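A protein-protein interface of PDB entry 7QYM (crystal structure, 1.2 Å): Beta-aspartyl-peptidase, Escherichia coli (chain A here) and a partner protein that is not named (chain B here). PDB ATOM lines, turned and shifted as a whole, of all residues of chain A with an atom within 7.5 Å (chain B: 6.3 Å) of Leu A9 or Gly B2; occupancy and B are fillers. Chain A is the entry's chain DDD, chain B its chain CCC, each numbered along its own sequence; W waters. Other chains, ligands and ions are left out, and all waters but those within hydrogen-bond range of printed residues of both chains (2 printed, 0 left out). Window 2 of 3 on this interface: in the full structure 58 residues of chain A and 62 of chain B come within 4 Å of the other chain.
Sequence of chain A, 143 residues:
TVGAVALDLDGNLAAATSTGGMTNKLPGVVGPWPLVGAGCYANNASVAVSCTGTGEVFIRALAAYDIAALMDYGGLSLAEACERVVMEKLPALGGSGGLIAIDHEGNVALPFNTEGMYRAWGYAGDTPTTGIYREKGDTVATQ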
ATOM      1  N   LEU A   7       0.142  11.232  19.793  1.00  0.00           N
ATOM      2  CA  LEU A   7      -1.209  10.679  19.651  1.00  0.00           C
ATOM      3  C   LEU A   7      -1.421  10.430  18.154  1.00  0.00           C
ATOM      4  O   LEU A   7      -1.235  11.348  17.374  1.00  0.00           O
ATOM      5  CB  LEU A   7      -2.220  11.690  20.169  1.00  0.00           C
ATOM      6  CG  LEU A   7      -3.677  11.317  19.945  1.00  0.00           C
ATOM      7  CD1 LEU A   7      -4.053  10.099  20.748  1.00  0.00           C
ATOM      8  CD2 LEU A   7      -4.532  12.476  20.369  1.00  0.00           C
ATOM      9  N   ASP A   8      -1.759   9.206  17.783  1.00  0.00           N
ATOM     10  CA  ASP A   8      -1.927   8.824  16.368  1.00  0.00           C
ATOM     11  C   ASP A   8      -3.373   8.869  15.928  1.00  0.00           C
ATOM     12  O   ASP A   8      -4.283   9.173  16.713  1.00  0.00           O
ATOM     13  CB  ASP A   8      -1.247   7.495  16.083  1.00  0.00           C
ATOM     14  CG  ASP A   8      -1.832   6.281  16.724  1.00  0.00           C
ATOM     15  OD1 ASP A   8      -3.062   6.308  16.981  1.00  0.00           O
ATOM     16  OD2 ASP A   8      -1.071   5.301  16.929  1.00  0.00           O
ATOM     17  N   LEU A   9      -3.610   8.704  14.641  1.00  0.00           N
ATOM     18  CA  LEU A   9      -4.963   8.747  14.073  1.00  0.00           C
ATOM     19  C   LEU A   9      -5.846   7.670  14.671  1.00  0.00           C
ATOM     20  O   LEU A   9      -7.080   7.841  14.559  1.00  0.00           O
ATOM     21  CB  LEU A   9      -4.918   8.585  12.549  1.00  0.00           C
ATOM     22  CG  LEU A   9      -4.303   9.762  11.801  1.00  0.00           C
ATOM     23  CD1 LEU A   9      -4.065   9.430  10.349  1.00  0.00           C
ATOM     24  CD2 LEU A   9      -5.078  11.040  11.974  1.00  0.00           C
ATOM     25  N   ASP A  10      -5.310   6.555  15.139  1.00  0.00           N
ATOM     26  CA  ASP A  10      -6.090   5.443  15.734  1.00  0.00           C
ATOM     27  C   ASP A  10      -6.461   5.759  17.188  1.00  0.00           C
ATOM     28  O   ASP A  10      -7.140   4.925  17.790  1.00  0.00           O
ATOM     29  CB  ASP A  10      -5.349   4.112  15.680  1.00  0.00           C
ATOM     30  CG  ASP A  10      -5.189   3.530  14.297  1.00  0.00           C
ATOM     31  OD1 ASP A  10      -6.114   3.677  13.492  1.00  0.00           O
ATOM     32  OD2 ASP A  10      -4.105   2.985  14.051  1.00  0.00           O
ATOM     33  N   GLY A  11      -5.960   6.861  17.762  1.00  0.00           N
ATOM     34  CA  GLY A  11      -6.261   7.263  19.150  1.00  0.00           C
ATOM     35  C   GLY A  11      -5.235   6.736  20.157  1.00  0.00           C
ATOM     36  O   GLY A  11      -5.504   6.727  21.368  1.00  0.00           O
ATOM     37  N   ASN A  12      -4.103   6.241  19.686  1.00  0.00           N
ATOM     38  CA  ASN A  12      -3.095   5.655  20.588  1.00  0.00           C
ATOM     39  C   ASN A  12      -2.055   6.686  20.984  1.00  0.00           C
ATOM     40  O   ASN A  12      -1.658   7.510  20.155  1.00  0.00           O
ATOM     41  CB  ASN A  12      -2.398   4.481  19.922  1.00  0.00           C
ATOM     42  CG  ASN A  12      -3.364   3.340  19.694  1.00  0.00           C
ATOM     43  OD1 ASN A  12      -4.187   3.003  20.539  1.00  0.00           O
ATOM     44  ND2 ASN A  12      -3.260   2.734  18.532  1.00  0.00           N
ATOM     45  N   GLU A 105      -7.294  13.240  24.565  1.00  0.00           N
ATOM     46  CA  GLU A 105      -8.152  14.189  23.810  1.00  0.00           C
ATOM     47  C   GLU A 105      -7.336  15.076  22.861  1.00  0.00           C
ATOM     48  O   GLU A 105      -7.935  15.888  22.170  1.00  0.00           O
ATOM     49  CB  GLU A 105      -9.001  14.956  24.829  1.00  0.00           C
ATOM     50  CG  GLU A 105     -10.033  14.021  25.461  1.00  0.00           C
ATOM     51  CD  GLU A 105     -10.647  14.456  26.777  1.00  0.00           C
ATOM     52  OE1 GLU A 105      -9.902  14.521  27.768  1.00  0.00           O
ATOM     53  OE2 GLU A 105     -11.876  14.699  26.808  1.00  0.00           O
ATOM     54  N   ALA A 124      -0.823  17.007  13.303  1.00  0.00           N
ATOM     55  CA  ALA A 124      -0.777  16.420  11.954  1.00  0.00           C
ATOM     56  C   ALA A 124      -1.565  17.362  11.041  1.00  0.00           C
ATOM     57  O   ALA A 124      -2.721  17.677  11.373  1.00  0.00           O
ATOM     58  CB  ALA A 124      -1.359  15.023  11.940  1.00  0.00           C
ATOM     59  N   GLY B   2      -9.112  10.752  14.851  1.00  0.00           N
ATOM     60  CA  GLY B   2      -9.027  11.956  15.741  1.00  0.00           C
ATOM     61  C   GLY B   2      -7.754  12.735  15.455  1.00  0.00           C
ATOM     62  O   GLY B   2      -6.940  12.214  14.630  1.00  0.00           O
ATOM     63  N   LYS B   3      -7.546  13.882  16.122  1.00  0.00           N
ATOM     64  CA  LYS B   3      -6.464  14.838  15.757  1.00  0.00           C
ATOM     65  C   LYS B   3      -5.100  14.371  16.292  1.00  0.00           C
ATOM     66  O   LYS B   3      -4.716  14.560  17.463  1.00  0.00           O
ATOM     67  CB  LYS B   3      -6.737  16.271  16.181  1.00  0.00           C
ATOM     68  CG  LYS B   3      -5.707  17.255  15.644  1.00  0.00           C
ATOM     69  CD  LYS B   3      -5.305  17.051  14.192  1.00  0.00           C
ATOM     70  CE  LYS B   3      -6.221  17.672  13.158  1.00  0.00           C
ATOM     71  NZ  LYS B   3      -5.584  17.699  11.810  1.00  0.00           N
ATOM     72  N   ALA B   4      -4.316  13.926  15.363  1.00  0.00           N
ATOM     73  CA  ALA B   4      -2.996  13.382  15.710  1.00  0.00           C
ATOM     74  C   ALA B   4      -2.032  14.531  15.980  1.00  0.00           C
ATOM     75  O   ALA B   4      -2.172  15.597  15.395  1.00  0.00           O
ATOM     76  CB  ALA B   4      -2.533  12.502  14.598  1.00  0.00           C
ATOM     77  N   LEU B  43       2.622  10.706  11.223  1.00  0.00           N
ATOM     78  CA  LEU B  43       1.269  10.608  11.828  1.00  0.00           C
ATOM     79  C   LEU B  43       0.218  10.769  10.721  1.00  0.00           C
ATOM     80  O   LEU B  43      -0.784  10.013  10.717  1.00  0.00           O
ATOM     81  CB  LEU B  43       1.109  11.664  12.900  1.00  0.00           C
ATOM     82  CG  LEU B  43       1.910  11.415  14.171  1.00  0.00           C
ATOM     83  CD1 LEU B  43       1.914  12.660  15.017  1.00  0.00           C
ATOM     84  CD2 LEU B  43       1.357  10.198  14.925  1.00  0.00           C
ATOM     85  N   GLU B  44       0.401  11.764   9.854  1.00  0.00           N
ATOM     86  CA  GLU B  44      -0.566  12.070   8.761  1.00  0.00           C
ATOM     87  C   GLU B  44      -0.708  10.833   7.866  1.00  0.00           C
ATOM     88  O   GLU B  44      -1.812  10.545   7.356  1.00  0.00           O
ATOM     89  CB  GLU B  44      -0.054  13.253   7.949  1.00  0.00           C
ATOM     90  CG  GLU B  44      -0.111  14.596   8.644  1.00  0.00           C
ATOM     91  CD  GLU B  44       0.819  15.645   8.042  1.00  0.00           C
ATOM     92  OE1 GLU B  44       1.112  15.523   6.831  1.00  0.00           O
ATOM     93  OE2 GLU B  44       1.277  16.570   8.787  1.00  0.00           O
ATOM     94  N   ALA B  45       0.360  10.069   7.703  1.00  0.00           N
ATOM     95  CA  ALA B  45       0.372   8.877   6.838  1.00  0.00           C
ATOM     96  C   ALA B  45      -0.110   7.612   7.568  1.00  0.00           C
ATOM     97  O   ALA B  45      -0.028   6.519   6.992  1.00  0.00           O
ATOM     98  CB  ALA B  45       1.775   8.667   6.296  1.00  0.00           C
ATOM     99  N   GLY B  46      -0.554   7.726   8.814  1.00  0.00           N
ATOM    100  CA  GLY B  46      -1.154   6.610   9.542  1.00  0.00           C
ATOM    101  C   GLY B  46      -0.160   5.767  10.278  1.00  0.00           C
ATOM    102  O   GLY B  46      -0.546   4.696  10.777  1.00  0.00           O
ATOM    103  N   GLU B  47       1.052   6.270  10.510  1.00  0.00           N
ATOM    104  CA  GLU B  47       2.025   5.536  11.324  1.00  0.00           C
ATOM    105  C   GLU B  47       1.601   5.614  12.784  1.00  0.00           C
ATOM    106  O   GLU B  47       0.909   6.567  13.189  1.00  0.00           O
ATOM    107  CB  GLU B  47       3.443   6.043  11.132  1.00  0.00           C
ATOM    108  CG  GLU B  47       3.949   5.842   9.727  1.00  0.00           C
ATOM    109  CD  GLU B  47       3.909   4.388   9.272  1.00  0.00           C
ATOM    110  OE1 GLU B  47       3.261   4.052   8.236  1.00  0.00           O
ATOM    111  OE2 GLU B  47       4.529   3.571   9.961  1.00  0.00           O
HETATM  112  O   HOH W   1      -6.435  10.807  17.459  1.00  0.00           O
HETATM  113  O   HOH W   2      -1.284   8.174  12.711  1.00  0.00           O
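The backbone carbonyl oxygen (O) of Ala B4 lies within hydrogen-bond range of the backbone NH (N) of Ala A124, 2.9 Å away.
NZ of Lys B3 sits at hydrogen-bond distance from O of Ala A124 (2.9 Å).
The side-chain carboxylate (OD1) of Asp A8 is in hydrogen-bond range of the backbone NH (N) of Asn A12, at 2.9 Å.
OD1 of Asp A8 is in hydrogen-bond range of N of Asp A10.
The side-chain carboxylate (OD1) of Asp A8 lies within hydrogen-bond range of the backbone NH (N) of Gly A11, 3.1 Å away.
Among the printed residues, pairs that only touch across the chains: Leu A7 with Lys B3, Leu A7 with Ala B4, Leu A7 with Leu B43, Asp A8 with Ala B4, Asp A8 with Leu B43, Asp A8 with Glu B47, Leu A9 with Gly B2, Leu A9 with Ala B4, Leu A9 with Leu B43, Leu A9 with Glu B44 and Ala A124 with Glu B44.
Leu A9 touches just these residues of chain B: Gly B2 (3.4 Å), Ala B4 (3.9 Å), Leu B43 (3.4 Å) and Glu B44 (3.9 Å).
Gly B2 touches just one residue of chain A: Leu A9.
Of the printed residues of chain A, Ala B4 touches Leu A7 (3.2 Å), Asp A8 (3.96 Å), Leu A9 (3.9 Å) and Ala A124 (2.9 Å).
Of the printed residues of chain A, Glu B47 touches Asp A8 (3.7 Å).
Of the printed residues of chain A, Lys B3 touches Leu A7 and Ala A124.
The nearest residue of chain B that does not touch Leu A9 is Gly B46 (4.1 Å).
The nearest printed residue of chain B that does not touch Asp A8 is Gly B2 (4.5 Å).
Printed residues of chain B that touch a printed residue of chain A: Gly B2, Lys B3, Ala B4, Leu B43, Glu B44 and Glu B47.
Along chain B the printed residues that touch a printed residue of chain A span positions 2 to 47.
Printed residues of chain A that touch a printed residue of chain B: Leu A7, Asp A8, Leu A9 and Ala A124.
Among the printed residues, 13 pairs touch across the chains.
Among the printed residues, no Asp or Glu carboxylate lies within 4 Å of a Lys or Arg side-chain nitrogen of the other chain.
Water W2 lies within hydrogen-bond range of O of Leu B43 (2.8 Å), O of Glu B47 (2.8 Å) and N of Leu A9 (3.1 Å).
Water W1 lies within hydrogen-bond range of O of Asp A8 (2.8 Å) and O of Gly B2 (3.2 Å).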
